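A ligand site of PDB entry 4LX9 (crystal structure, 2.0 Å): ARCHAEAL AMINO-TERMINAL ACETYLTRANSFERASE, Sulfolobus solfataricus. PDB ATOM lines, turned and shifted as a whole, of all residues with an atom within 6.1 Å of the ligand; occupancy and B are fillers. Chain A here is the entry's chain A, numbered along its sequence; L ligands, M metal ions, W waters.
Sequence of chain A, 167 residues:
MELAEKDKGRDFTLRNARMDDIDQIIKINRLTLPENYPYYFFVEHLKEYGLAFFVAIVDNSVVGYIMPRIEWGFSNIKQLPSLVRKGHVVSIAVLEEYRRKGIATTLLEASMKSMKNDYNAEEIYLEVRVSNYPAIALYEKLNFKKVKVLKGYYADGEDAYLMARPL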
ATOM      1  N   THR A  32     -27.781 -20.464 -18.359  1.00  0.00           N
ATOM      2  CA  THR A  32     -26.980 -21.522 -19.006  1.00  0.00           C
ATOM      3  C   THR A  32     -27.378 -22.978 -18.696  1.00  0.00           C
ATOM      4  O   THR A  32     -26.876 -23.893 -19.348  1.00  0.00           O
ATOM      5  CB  THR A  32     -25.477 -21.398 -18.652  1.00  0.00           C
ATOM      6  OG1 THR A  32     -25.306 -21.553 -17.240  1.00  0.00           O
ATOM      7  CG2 THR A  32     -24.936 -20.047 -19.079  1.00  0.00           C
ATOM      8  N   LEU A  33     -28.245 -23.192 -17.713  1.00  0.00           N
ATOM      9  CA  LEU A  33     -28.586 -24.529 -17.246  1.00  0.00           C
ATOM     10  C   LEU A  33     -30.057 -24.612 -16.850  1.00  0.00           C
ATOM     11  O   LEU A  33     -30.653 -23.602 -16.473  1.00  0.00           O
ATOM     12  CB  LEU A  33     -27.705 -24.895 -16.041  1.00  0.00           C
ATOM     13  CG  LEU A  33     -26.207 -25.107 -16.228  1.00  0.00           C
ATOM     14  CD1 LEU A  33     -25.484 -25.006 -14.874  1.00  0.00           C
ATOM     15  CD2 LEU A  33     -25.900 -26.460 -16.894  1.00  0.00           C
ATOM     16  N   VAL A  89     -18.210 -31.571  -8.147  1.00  0.00           N
ATOM     17  CA  VAL A  89     -18.538 -30.354  -8.893  1.00  0.00           C
ATOM     18  C   VAL A  89     -20.038 -30.315  -9.085  1.00  0.00           C
ATOM     19  O   VAL A  89     -20.597 -30.971  -9.969  1.00  0.00           O
ATOM     20  CB  VAL A  89     -17.844 -30.281 -10.249  1.00  0.00           C
ATOM     21  CG1 VAL A  89     -18.045 -28.879 -10.875  1.00  0.00           C
ATOM     22  CG2 VAL A  89     -16.358 -30.609 -10.108  1.00  0.00           C
ATOM     23  N   VAL A  90     -20.705 -29.563  -8.217  1.00  0.00           N
ATOM     24  CA  VAL A  90     -22.159 -29.489  -8.243  1.00  0.00           C
ATOM     25  C   VAL A  90     -22.603 -28.740  -9.488  1.00  0.00           C
ATOM     26  O   VAL A  90     -23.505 -29.179 -10.208  1.00  0.00           O
ATOM     27  CB  VAL A  90     -22.690 -28.800  -6.980  1.00  0.00           C
ATOM     28  CG1 VAL A  90     -24.221 -28.732  -7.017  1.00  0.00           C
ATOM     29  CG2 VAL A  90     -22.203 -29.533  -5.736  1.00  0.00           C
ATOM     30  N   SER A  91     -21.938 -27.621  -9.761  1.00  0.00           N
ATOM     31  CA  SER A  91     -22.290 -26.819 -10.916  1.00  0.00           C
ATOM     32  C   SER A  91     -21.091 -26.005 -11.426  1.00  0.00           C
ATOM     33  O   SER A  91     -20.214 -25.589 -10.658  1.00  0.00           O
ATOM     34  CB  SER A  91     -23.450 -25.875 -10.567  1.00  0.00           C
ATOM     35  OG  SER A  91     -23.948 -25.250 -11.733  1.00  0.00           O
ATOM     36  N   ILE A  92     -21.056 -25.806 -12.738  1.00  0.00           N
ATOM     37  CA  ILE A  92     -20.068 -24.933 -13.356  1.00  0.00           C
ATOM     38  C   ILE A  92     -20.637 -24.380 -14.665  1.00  0.00           C
ATOM     39  O   ILE A  92     -21.283 -25.098 -15.441  1.00  0.00           O
ATOM     40  CB  ILE A  92     -18.727 -25.663 -13.603  1.00  0.00           C
ATOM     41  CG1 ILE A  92     -17.748 -24.744 -14.353  1.00  0.00           C
ATOM     42  CG2 ILE A  92     -18.945 -26.981 -14.370  1.00  0.00           C
ATOM     43  CD1 ILE A  92     -16.328 -25.271 -14.434  1.00  0.00           C
ATOM     44  N   ALA A  93     -20.403 -23.097 -14.916  1.00  0.00           N
ATOM     45  CA  ALA A  93     -20.941 -22.452 -16.102  1.00  0.00           C
ATOM     46  C   ALA A  93     -20.172 -21.189 -16.424  1.00  0.00           C
ATOM     47  O   ALA A  93     -19.591 -20.562 -15.535  1.00  0.00           O
ATOM     48  CB  ALA A  93     -22.410 -22.130 -15.884  1.00  0.00           C
ATOM     49  N   VAL A  94     -20.176 -20.827 -17.701  1.00  0.00           N
ATOM     50  CA  VAL A  94     -19.509 -19.624 -18.192  1.00  0.00           C
ATOM     51  C   VAL A  94     -20.439 -18.974 -19.198  1.00  0.00           C
ATOM     52  O   VAL A  94     -21.025 -19.666 -20.021  1.00  0.00           O
ATOM     53  CB  VAL A  94     -18.176 -19.987 -18.901  1.00  0.00           C
ATOM     54  CG1 VAL A  94     -17.566 -18.758 -19.555  1.00  0.00           C
ATOM     55  CG2 VAL A  94     -17.205 -20.607 -17.917  1.00  0.00           C
ATOM     56  N   LEU A  95     -20.617 -17.661 -19.097  1.00  0.00           N
ATOM     57  CA  LEU A  95     -21.478 -16.954 -20.045  1.00  0.00           C
ATOM     58  C   LEU A  95     -21.014 -17.228 -21.476  1.00  0.00           C
ATOM     59  O   LEU A  95     -19.817 -17.323 -21.742  1.00  0.00           O
ATOM     60  CB  LEU A  95     -21.518 -15.449 -19.745  1.00  0.00           C
ATOM     61  CG  LEU A  95     -22.324 -15.030 -18.507  1.00  0.00           C
ATOM     62  CD1 LEU A  95     -22.179 -13.533 -18.220  1.00  0.00           C
ATOM     63  CD2 LEU A  95     -23.787 -15.405 -18.656  1.00  0.00           C
ATOM     64  N   TYR A  98     -18.174 -15.489 -23.351  1.00  0.00           N
ATOM     65  CA  TYR A  98     -16.826 -15.673 -22.817  1.00  0.00           C
ATOM     66  C   TYR A  98     -16.344 -17.122 -22.843  1.00  0.00           C
ATOM     67  O   TYR A  98     -15.421 -17.480 -22.131  1.00  0.00           O
ATOM     68  CB  TYR A  98     -16.722 -15.108 -21.403  1.00  0.00           C
ATOM     69  CG  TYR A  98     -17.106 -13.648 -21.331  1.00  0.00           C
ATOM     70  CD1 TYR A  98     -16.206 -12.659 -21.699  1.00  0.00           C
ATOM     71  CD2 TYR A  98     -18.370 -13.271 -20.915  1.00  0.00           C
ATOM     72  CE1 TYR A  98     -16.554 -11.322 -21.653  1.00  0.00           C
ATOM     73  CE2 TYR A  98     -18.722 -11.928 -20.854  1.00  0.00           C
ATOM     74  CZ  TYR A  98     -17.806 -10.967 -21.224  1.00  0.00           C
ATOM     75  OH  TYR A  98     -18.154  -9.631 -21.179  1.00  0.00           O
ATOM     76  N   ARG A  99     -16.985 -17.952 -23.672  1.00  0.00           N
ATOM     77  CA  ARG A  99     -16.614 -19.352 -23.800  1.00  0.00           C
ATOM     78  C   ARG A  99     -15.407 -19.574 -24.721  1.00  0.00           C
ATOM     79  O   ARG A  99     -14.991 -18.658 -25.457  1.00  0.00           O
ATOM     80  CB  ARG A  99     -17.818 -20.184 -24.244  1.00  0.00           C
ATOM     81  CG  ARG A  99     -18.830 -20.403 -23.109  1.00  0.00           C
ATOM     82  CD  ARG A  99     -20.077 -21.148 -23.551  1.00  0.00           C
ATOM     83  NE  ARG A  99     -21.126 -21.040 -22.531  1.00  0.00           N
ATOM     84  CZ  ARG A  99     -22.392 -21.386 -22.718  1.00  0.00           C
ATOM     85  NH1 ARG A  99     -22.784 -21.866 -23.889  1.00  0.00           N
ATOM     86  NH2 ARG A  99     -23.274 -21.222 -21.738  1.00  0.00           N
ATOM     87  N   ARG A 100     -14.845 -20.775 -24.660  1.00  0.00           N
ATOM     88  CA  ARG A 100     -13.667 -21.182 -25.442  1.00  0.00           C
ATOM     89  C   ARG A 100     -12.407 -20.362 -25.167  1.00  0.00           C
ATOM     90  O   ARG A 100     -11.525 -20.294 -26.023  1.00  0.00           O
ATOM     91  CB  ARG A 100     -13.930 -21.150 -26.954  1.00  0.00           C
ATOM     92  CG  ARG A 100     -14.986 -22.106 -27.473  1.00  0.00           C
ATOM     93  CD  ARG A 100     -14.815 -23.514 -26.936  1.00  0.00           C
ATOM     94  NE  ARG A 100     -13.745 -24.290 -27.565  1.00  0.00           N
ATOM     95  CZ  ARG A 100     -13.863 -24.960 -28.709  1.00  0.00           C
ATOM     96  NH1 ARG A 100     -14.991 -24.938 -29.392  1.00  0.00           N
ATOM     97  NH2 ARG A 100     -12.823 -25.638 -29.174  1.00  0.00           N
ATOM     98  N   LYS A 101     -12.315 -19.752 -23.990  1.00  0.00           N
ATOM     99  CA  LYS A 101     -11.149 -18.933 -23.655  1.00  0.00           C
ATOM    100  C   LYS A 101     -10.348 -19.541 -22.513  1.00  0.00           C
ATOM    101  O   LYS A 101      -9.368 -18.970 -22.066  1.00  0.00           O
ATOM    102  CB  LYS A 101     -11.591 -17.504 -23.298  1.00  0.00           C
ATOM    103  CG  LYS A 101     -12.177 -16.723 -24.472  1.00  0.00           C
ATOM    104  CD  LYS A 101     -13.118 -15.580 -24.023  1.00  0.00           C
ATOM    105  CE  LYS A 101     -12.372 -14.448 -23.320  1.00  0.00           C
ATOM    106  NZ  LYS A 101     -11.406 -13.746 -24.232  1.00  0.00           N
ATOM    107  N   GLY A 102     -10.776 -20.707 -22.027  1.00  0.00           N
ATOM    108  CA  GLY A 102     -10.030 -21.413 -20.994  1.00  0.00           C
ATOM    109  C   GLY A 102     -10.497 -21.102 -19.592  1.00  0.00           C
ATOM    110  O   GLY A 102      -9.850 -21.451 -18.606  1.00  0.00           O
ATOM    111  N   ILE A 103     -11.657 -20.445 -19.506  1.00  0.00           N
ATOM    112  CA  ILE A 103     -12.192 -20.028 -18.215  1.00  0.00           C
ATOM    113  C   ILE A 103     -12.666 -21.222 -17.345  1.00  0.00           C
ATOM    114  O   ILE A 103     -12.384 -21.260 -16.157  1.00  0.00           O
ATOM    115  CB  ILE A 103     -13.326 -18.998 -18.397  1.00  0.00           C
ATOM    116  CG1 ILE A 103     -12.757 -17.669 -18.904  1.00  0.00           C
ATOM    117  CG2 ILE A 103     -14.048 -18.777 -17.094  1.00  0.00           C
ATOM    118  CD1 ILE A 103     -13.814 -16.642 -19.292  1.00  0.00           C
ATOM    119  N   ALA A 104     -13.376 -22.176 -17.943  1.00  0.00           N
ATOM    120  CA  ALA A 104     -13.878 -23.307 -17.154  1.00  0.00           C
ATOM    121  C   ALA A 104     -12.729 -24.209 -16.726  1.00  0.00           C
ATOM    122  O   ALA A 104     -12.753 -24.771 -15.647  1.00  0.00           O
ATOM    123  CB  ALA A 104     -14.951 -24.104 -17.917  1.00  0.00           C
ATOM    124  N   THR A 105     -11.730 -24.330 -17.597  1.00  0.00           N
ATOM    125  CA  THR A 105     -10.526 -25.102 -17.284  1.00  0.00           C
ATOM    126  C   THR A 105      -9.872 -24.536 -16.043  1.00  0.00           C
ATOM    127  O   THR A 105      -9.600 -25.267 -15.091  1.00  0.00           O
ATOM    128  CB  THR A 105      -9.533 -25.053 -18.452  1.00  0.00           C
ATOM    129  OG1 THR A 105     -10.138 -25.606 -19.627  1.00  0.00           O
ATOM    130  CG2 THR A 105      -8.245 -25.829 -18.121  1.00  0.00           C
ATOM    131  N   THR A 106      -9.643 -23.227 -16.060  1.00  0.00           N
ATOM    132  CA  THR A 106      -9.037 -22.523 -14.926  1.00  0.00           C
ATOM    133  C   THR A 106      -9.869 -22.636 -13.655  1.00  0.00           C
ATOM    134  O   THR A 106      -9.342 -22.854 -12.563  1.00  0.00           O
ATOM    135  CB  THR A 106      -8.834 -21.034 -15.251  1.00  0.00           C
ATOM    136  OG1 THR A 106      -8.147 -20.900 -16.498  1.00  0.00           O
ATOM    137  CG2 THR A 106      -8.011 -20.368 -14.165  1.00  0.00           C
ATOM    138  N   LEU A 126     -18.629 -35.759 -10.856  1.00  0.00           N
ATOM    139  CA  LEU A 126     -19.757 -34.947 -11.284  1.00  0.00           C
ATOM    140  C   LEU A 126     -20.658 -35.770 -12.184  1.00  0.00           C
ATOM    141  O   LEU A 126     -20.280 -36.844 -12.610  1.00  0.00           O
ATOM    142  CB  LEU A 126     -19.261 -33.710 -12.043  1.00  0.00           C
ATOM    143  CG  LEU A 126     -18.360 -34.001 -13.255  1.00  0.00           C
ATOM    144  CD1 LEU A 126     -19.176 -34.182 -14.558  1.00  0.00           C
ATOM    145  CD2 LEU A 126     -17.279 -32.950 -13.421  1.00  0.00           C
ATOM    146  N   GLU A 127     -21.854 -35.250 -12.463  1.00  0.00           N
ATOM    147  CA  GLU A 127     -22.721 -35.811 -13.483  1.00  0.00           C
ATOM    148  C   GLU A 127     -22.853 -34.795 -14.608  1.00  0.00           C
ATOM    149  O   GLU A 127     -22.794 -33.585 -14.373  1.00  0.00           O
ATOM    150  CB  GLU A 127     -24.103 -36.148 -12.938  1.00  0.00           C
ATOM    151  CG  GLU A 127     -24.114 -36.869 -11.565  1.00  0.00           C
ATOM    152  CD  GLU A 127     -23.897 -35.917 -10.390  1.00  0.00           C
ATOM    153  OE1 GLU A 127     -24.221 -34.725 -10.533  1.00  0.00           O
ATOM    154  OE2 GLU A 127     -23.399 -36.358  -9.331  1.00  0.00           O
ATOM    155  N   VAL A 128     -23.030 -35.294 -15.824  1.00  0.00           N
ATOM    156  CA  VAL A 128     -23.191 -34.421 -16.972  1.00  0.00           C
ATOM    157  C   VAL A 128     -24.099 -35.113 -17.970  1.00  0.00           C
ATOM    158  O   VAL A 128     -23.998 -36.329 -18.141  1.00  0.00           O
ATOM    159  CB  VAL A 128     -21.837 -34.077 -17.617  1.00  0.00           C
ATOM    160  CG1 VAL A 128     -21.022 -35.352 -17.930  1.00  0.00           C
ATOM    161  CG2 VAL A 128     -22.017 -33.205 -18.873  1.00  0.00           C
ATOM    162  N   ARG A 129     -24.997 -34.351 -18.589  1.00  0.00           N
ATOM    163  CA  ARG A 129     -25.849 -34.881 -19.650  1.00  0.00           C
ATOM    164  C   ARG A 129     -25.014 -35.509 -20.743  1.00  0.00           C
ATOM    165  O   ARG A 129     -23.987 -34.958 -21.164  1.00  0.00           O
ATOM    166  CB  ARG A 129     -26.692 -33.757 -20.258  1.00  0.00           C
ATOM    167  CG  ARG A 129     -27.740 -33.202 -19.325  1.00  0.00           C
ATOM    168  CD  ARG A 129     -28.550 -32.055 -19.927  1.00  0.00           C
ATOM    169  NE  ARG A 129     -29.489 -31.548 -18.951  1.00  0.00           N
ATOM    170  CZ  ARG A 129     -30.712 -32.046 -18.755  1.00  0.00           C
ATOM    171  NH1 ARG A 129     -31.155 -33.058 -19.483  1.00  0.00           N
ATOM    172  NH2 ARG A 129     -31.493 -31.527 -17.807  1.00  0.00           N
ATOM    173  N   ASN A 132     -24.016 -33.321 -23.626  1.00  0.00           N
ATOM    174  CA  ASN A 132     -23.253 -32.114 -23.354  1.00  0.00           C
ATOM    175  C   ASN A 132     -21.798 -32.290 -23.795  1.00  0.00           C
ATOM    176  O   ASN A 132     -20.890 -32.375 -22.967  1.00  0.00           O
ATOM    177  CB  ASN A 132     -23.358 -31.740 -21.866  1.00  0.00           C
ATOM    178  CG  ASN A 132     -22.872 -30.329 -21.581  1.00  0.00           C
ATOM    179  OD1 ASN A 132     -22.225 -29.706 -22.419  1.00  0.00           O
ATOM    180  ND2 ASN A 132     -23.158 -29.827 -20.379  1.00  0.00           N
ATOM    181  N   TYR A 133     -21.572 -32.348 -25.106  1.00  0.00           N
ATOM    182  CA  TYR A 133     -20.222 -32.541 -25.626  1.00  0.00           C
ATOM    183  C   TYR A 133     -19.173 -31.487 -25.197  1.00  0.00           C
ATOM    184  O   TYR A 133     -18.009 -31.839 -25.008  1.00  0.00           O
ATOM    185  CB  TYR A 133     -20.236 -32.715 -27.156  1.00  0.00           C
ATOM    186  CG  TYR A 133     -20.645 -31.465 -27.906  1.00  0.00           C
ATOM    187  CD1 TYR A 133     -19.689 -30.610 -28.447  1.00  0.00           C
ATOM    188  CD2 TYR A 133     -21.984 -31.144 -28.082  1.00  0.00           C
ATOM    189  CE1 TYR A 133     -20.057 -29.471 -29.130  1.00  0.00           C
ATOM    190  CE2 TYR A 133     -22.358 -29.994 -28.772  1.00  0.00           C
ATOM    191  CZ  TYR A 133     -21.384 -29.163 -29.292  1.00  0.00           C
ATOM    192  OH  TYR A 133     -21.730 -28.021 -29.977  1.00  0.00           O
ATOM    193  N   PRO A 134     -19.578 -30.207 -25.051  1.00  0.00           N
ATOM    194  CA  PRO A 134     -18.537 -29.266 -24.620  1.00  0.00           C
ATOM    195  C   PRO A 134     -18.039 -29.540 -23.206  1.00  0.00           C
ATOM    196  O   PRO A 134     -16.844 -29.450 -22.957  1.00  0.00           O
ATOM    197  CB  PRO A 134     -19.235 -27.908 -24.670  1.00  0.00           C
ATOM    198  CG  PRO A 134     -20.374 -28.090 -25.623  1.00  0.00           C
ATOM    199  CD  PRO A 134     -20.836 -29.488 -25.336  1.00  0.00           C
ATOM    200  N   ALA A 135     -18.967 -29.858 -22.305  1.00  0.00           N
ATOM    201  CA  ALA A 135     -18.607 -30.131 -20.921  1.00  0.00           C
ATOM    202  C   ALA A 135     -17.826 -31.446 -20.836  1.00  0.00           C
ATOM    203  O   ALA A 135     -16.761 -31.504 -20.212  1.00  0.00           O
ATOM    204  CB  ALA A 135     -19.835 -30.176 -20.056  1.00  0.00           C
ATOM    205  N   ALA A 137     -16.028 -32.867 -23.111  1.00  0.00           N
ATOM    206  CA  ALA A 137     -14.683 -32.587 -23.639  1.00  0.00           C
ATOM    207  C   ALA A 137     -13.826 -31.892 -22.584  1.00  0.00           C
ATOM    208  O   ALA A 137     -12.665 -32.246 -22.381  1.00  0.00           O
ATOM    209  CB  ALA A 137     -14.779 -31.736 -24.904  1.00  0.00           C
ATOM    210  N   LEU A 138     -14.411 -30.909 -21.906  1.00  0.00           N
ATOM    211  CA  LEU A 138     -13.727 -30.168 -20.865  1.00  0.00           C
ATOM    212  C   LEU A 138     -13.210 -31.112 -19.787  1.00  0.00           C
ATOM    213  O   LEU A 138     -12.036 -31.074 -19.435  1.00  0.00           O
ATOM    214  CB  LEU A 138     -14.670 -29.134 -20.226  1.00  0.00           C
ATOM    215  CG  LEU A 138     -14.342 -28.626 -18.819  1.00  0.00           C
ATOM    216  CD1 LEU A 138     -13.083 -27.756 -18.799  1.00  0.00           C
ATOM    217  CD2 LEU A 138     -15.559 -27.883 -18.208  1.00  0.00           C
ATOM    218  N   TYR A 139     -14.100 -31.948 -19.250  1.00  0.00           N
ATOM    219  CA  TYR A 139     -13.750 -32.867 -18.181  1.00  0.00           C
ATOM    220  C   TYR A 139     -12.686 -33.873 -18.632  1.00  0.00           C
ATOM    221  O   TYR A 139     -11.711 -34.101 -17.924  1.00  0.00           O
ATOM    222  CB  TYR A 139     -14.994 -33.596 -17.655  1.00  0.00           C
ATOM    223  CG  TYR A 139     -16.083 -32.644 -17.207  1.00  0.00           C
ATOM    224  CD1 TYR A 139     -15.758 -31.450 -16.583  1.00  0.00           C
ATOM    225  CD2 TYR A 139     -17.424 -32.912 -17.468  1.00  0.00           C
ATOM    226  CE1 TYR A 139     -16.735 -30.566 -16.192  1.00  0.00           C
ATOM    227  CE2 TYR A 139     -18.407 -32.027 -17.085  1.00  0.00           C
ATOM    228  CZ  TYR A 139     -18.057 -30.867 -16.434  1.00  0.00           C
ATOM    229  OH  TYR A 139     -19.024 -29.969 -16.059  1.00  0.00           O
ATOM    230  N   LYS A 141     -10.481 -33.583 -20.892  1.00  0.00           N
ATOM    231  CA  LYS A 141      -9.224 -32.853 -21.045  1.00  0.00           C
ATOM    232  C   LYS A 141      -8.519 -32.660 -19.704  1.00  0.00           C
ATOM    233  O   LYS A 141      -7.301 -32.592 -19.640  1.00  0.00           O
ATOM    234  CB  LYS A 141      -9.465 -31.520 -21.761  1.00  0.00           C
ATOM    235  CG  LYS A 141      -8.207 -30.742 -22.110  1.00  0.00           C
ATOM    236  CD  LYS A 141      -8.477 -29.742 -23.233  1.00  0.00           C
ATOM    237  CE  LYS A 141      -8.217 -30.369 -24.601  1.00  0.00           C
ATOM    238  NZ  LYS A 141      -8.271 -29.357 -25.717  1.00  0.00           N
ATOM    239  N   TYR A 154     -31.708 -37.067 -15.323  1.00  0.00           N
ATOM    240  CA  TYR A 154     -32.257 -35.712 -15.325  1.00  0.00           C
ATOM    241  C   TYR A 154     -33.780 -35.714 -15.317  1.00  0.00           C
ATOM    242  O   TYR A 154     -34.411 -36.721 -15.649  1.00  0.00           O
ATOM    243  CB  TYR A 154     -31.665 -34.891 -16.473  1.00  0.00           C
ATOM    244  CG  TYR A 154     -30.196 -34.583 -16.241  1.00  0.00           C
ATOM    245  CD1 TYR A 154     -29.809 -33.462 -15.523  1.00  0.00           C
ATOM    246  CD2 TYR A 154     -29.214 -35.443 -16.693  1.00  0.00           C
ATOM    247  CE1 TYR A 154     -28.461 -33.198 -15.291  1.00  0.00           C
ATOM    248  CE2 TYR A 154     -27.892 -35.191 -16.469  1.00  0.00           C
ATOM    249  CZ  TYR A 154     -27.514 -34.078 -15.770  1.00  0.00           C
ATOM    250  OH  TYR A 154     -26.176 -33.821 -15.556  1.00  0.00           O
HETATM  251  N1  LIG L   1     -17.074 -27.884 -28.525  1.00  0.00           N
HETATM  252  C1  LIG L   1     -16.104 -28.781 -28.328  1.00  0.00           C
HETATM  253  N2  LIG L   1     -15.273 -28.702 -27.274  1.00  0.00           N
HETATM  254  C2  LIG L   1     -15.418 -27.718 -26.364  1.00  0.00           C
HETATM  255  C3  LIG L   1     -16.416 -26.750 -26.522  1.00  0.00           C
HETATM  256  C4  LIG L   1     -17.242 -26.875 -27.644  1.00  0.00           C
HETATM  257  N3  LIG L   1     -18.261 -25.951 -27.854  1.00  0.00           N
HETATM  258  N4  LIG L   1     -16.323 -25.878 -25.480  1.00  0.00           N
HETATM  259  C5  LIG L   1     -15.295 -26.298 -24.699  1.00  0.00           C
HETATM  260  N5  LIG L   1     -14.749 -27.415 -25.237  1.00  0.00           N
HETATM  261  C6  LIG L   1     -13.617 -28.203 -24.773  1.00  0.00           C
HETATM  262  C7  LIG L   1     -12.407 -27.912 -25.595  1.00  0.00           C
HETATM  263  O1  LIG L   1     -11.653 -29.068 -25.711  1.00  0.00           O
HETATM  264  C8  LIG L   1     -11.691 -26.953 -24.810  1.00  0.00           C
HETATM  265  O2  LIG L   1     -10.333 -26.919 -25.175  1.00  0.00           O
HETATM  266  P1  LIG L   1      -9.839 -26.413 -26.598  1.00  0.00           P
HETATM  267  O3  LIG L   1     -10.913 -25.747 -27.402  1.00  0.00           O
HETATM  268  O4  LIG L   1      -9.368 -27.651 -27.343  1.00  0.00           O
HETATM  269  O5  LIG L   1      -8.663 -25.492 -26.364  1.00  0.00           O
HETATM  270  C9  LIG L   1     -11.916 -27.448 -23.450  1.00  0.00           C
HETATM  271  O6  LIG L   1     -13.252 -27.972 -23.448  1.00  0.00           O
HETATM  272  C10 LIG L   1     -11.842 -26.377 -22.443  1.00  0.00           C
HETATM  273  O7  LIG L   1     -12.487 -25.211 -22.790  1.00  0.00           O
HETATM  274  P2  LIG L   1     -12.759 -24.020 -21.796  1.00  0.00           P
HETATM  275  O8  LIG L   1     -12.533 -22.713 -22.540  1.00  0.00           O
HETATM  276  O9  LIG L   1     -11.880 -24.094 -20.565  1.00  0.00           O
HETATM  277  O10 LIG L   1     -14.326 -24.173 -21.408  1.00  0.00           O
HETATM  278  P3  LIG L   1     -15.378 -22.947 -21.343  1.00  0.00           P
HETATM  279  O11 LIG L   1     -14.716 -21.769 -20.663  1.00  0.00           O
HETATM  280  O12 LIG L   1     -15.881 -22.561 -22.704  1.00  0.00           O
HETATM  281  O13 LIG L   1     -16.590 -23.481 -20.538  1.00  0.00           O
HETATM  282  C11 LIG L   1     -18.477 -24.990 -20.415  1.00  0.00           C
HETATM  283  C12 LIG L   1     -17.069 -24.729 -20.867  1.00  0.00           C
HETATM  284  C13 LIG L   1     -18.843 -26.418 -20.647  1.00  0.00           C
HETATM  285  C14 LIG L   1     -18.575 -24.701 -18.907  1.00  0.00           C
HETATM  286  C15 LIG L   1     -19.442 -24.028 -21.204  1.00  0.00           C
HETATM  287  O14 LIG L   1     -19.582 -24.509 -22.489  1.00  0.00           O
HETATM  288  C16 LIG L   1     -20.803 -23.745 -20.571  1.00  0.00           C
HETATM  289  O15 LIG L   1     -20.937 -22.889 -19.731  1.00  0.00           O
HETATM  290  N6  LIG L   1     -21.974 -24.539 -20.984  1.00  0.00           N
HETATM  291  C17 LIG L   1     -23.272 -24.305 -20.384  1.00  0.00           C
HETATM  292  C18 LIG L   1     -23.380 -24.790 -18.907  1.00  0.00           C
HETATM  293  C19 LIG L   1     -22.883 -26.234 -18.632  1.00  0.00           C
HETATM  294  O16 LIG L   1     -23.055 -27.126 -19.459  1.00  0.00           O
HETATM  295  N7  LIG L   1     -22.204 -26.516 -17.394  1.00  0.00           N
HETATM  296  C20 LIG L   1     -21.763 -27.874 -17.120  1.00  0.00           C
HETATM  297  C21 LIG L   1     -22.870 -28.842 -16.712  1.00  0.00           C
HETATM  298  S1  LIG L   1     -22.344 -30.304 -15.812  1.00  0.00           S
HETATM  299  C22 LIG L   1     -21.467 -29.609 -14.375  1.00  0.00           C
HETATM  300  O17 LIG L   1     -22.240 -28.565 -13.903  1.00  0.00           O
HETATM  301  C23 LIG L   1     -21.177 -30.595 -13.312  1.00  0.00           C
HETATM  302 ZN    ZN M   1     -23.673 -33.532  -9.157  1.00  0.00          ZN
HETATM  303  O   HOH W   1     -22.247 -32.667 -10.798  1.00  0.00           O
HETATM  304  O   HOH W   2     -24.162 -31.791 -12.565  1.00  0.00           O
HETATM  305  O   HOH W   3     -18.900 -23.330 -26.516  1.00  0.00           O
HETATM  306  O   HOH W   4     -17.561 -23.726 -24.068  1.00  0.00           O
HETATM  307  O   HOH W   5     -22.344 -26.780 -22.773  1.00  0.00           O
HETATM  308  O   HOH W   6     -13.795 -19.713 -21.496  1.00  0.00           O
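The backbone carbonyl oxygen (O) of Glu 127 lies close to a sulfur (S1) of the ligand (3.6 Å).
O of Thr 32 touches C18 of the ligand, at 3.6 Å.
Leu 33 touches the ligand.
Val 89 touches the ligand.
Val 90 touches the ligand.
CA of Ser 91 touches O17 of the ligand, 3.5 Å away.
Ala 93 touches the ligand (CA to O15, 3.7 Å).
N of Ile 103 touches O11 of the ligand (3.5 Å).
CB of Leu 126 touches C23 of the ligand (3.9 Å).
CE1 of Tyr 133 touches N1 of the ligand, 3.4 Å away.
Pro 134 touches the ligand.
Ala 135 touches the ligand.
Ala 137 touches the ligand.
Leu 138 touches the ligand.
25 residues have an atom within 4 Å of the ligand: Thr 32, Leu 33, Val 89, Val 90, Ser 91, Ile 92, Ala 93, Val 94, Arg 99, Arg 100, Lys 101, Gly 102, Ile 103, Ala 104, Thr 105, Leu 126, Glu 127, Asn 132, Tyr 133, Pro 134, Ala 135, Ala 137, Leu 138, Tyr 139 and Lys 141.
The nearest printed residue that does not touch the ligand is Val 128 (4.2 Å).
OG1 of Thr 106 lies within hydrogen-bond range of O of Gly 102 (2.8 Å).
The side-chain amide oxygen (OD1) of Asn 132 is in hydrogen-bond range of the backbone NH (N) of Ala 135, at 3.3 Å.
The backbone carbonyl oxygen (O) of Val 94 sits at hydrogen-bond distance from the guanidinium group (NE) of Arg 99 (2.9 Å).
N of Thr 105 lies within hydrogen-bond range of O9 of the ligand (3.0 Å).
O9 of the ligand lies within hydrogen-bond range of OG1 of Thr 105 (2.5 Å).
The backbone NH (N) of Ile 92 sits at hydrogen-bond distance from an oxygen (O17) of the ligand (3.2 Å).
The backbone carbonyl oxygen of Ile 92 is in hydrogen-bond range of a nitrogen (N7) of the ligand (2.6 Å).
The side-chain amino group of Lys 141 lies within salt-bridge range of an oxygen (O4) of the ligand, at 2.6 Å.
The backbone NH (N) of Arg 100 sits at hydrogen-bond distance from an oxygen (O12) of the ligand.
The guanidinium group (NH2) of Arg 100 lies within salt-bridge range of an oxygen (O3) of the ligand (2.6 Å).
An oxygen (O8) of the ligand is in hydrogen-bond range of the backbone NH (N) of Gly 102 (2.7 Å).
O16 of the ligand sits at hydrogen-bond distance from ND2 of Asn 132 (2.9 Å).
The side-chain hydroxyl (OH) of Tyr 139 lies close to a sulfur (S1) of the ligand (3.3 Å).
The backbone NH (N) of Val 94 lies within hydrogen-bond range of an oxygen (O15) of the ligand (3.0 Å).
N of Ala 104 lies within hydrogen-bond range of O11 of the ligand, at 3.1 Å.
The backbone NH of Lys 101 is in hydrogen-bond range of an oxygen (O8) of the ligand, 3.3 Å away.
The guanidinium group of Arg 99 sits close to an oxygen (O15) of the ligand (3.4 Å).
Water W5 bridges a nitrogen (N6) of the ligand (2.9 Å) and the side-chain amide oxygen (OD1) of Asn 132 (2.9 Å).
Water W1 lies within hydrogen-bond range of O of Val 89 and N of Glu 127.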
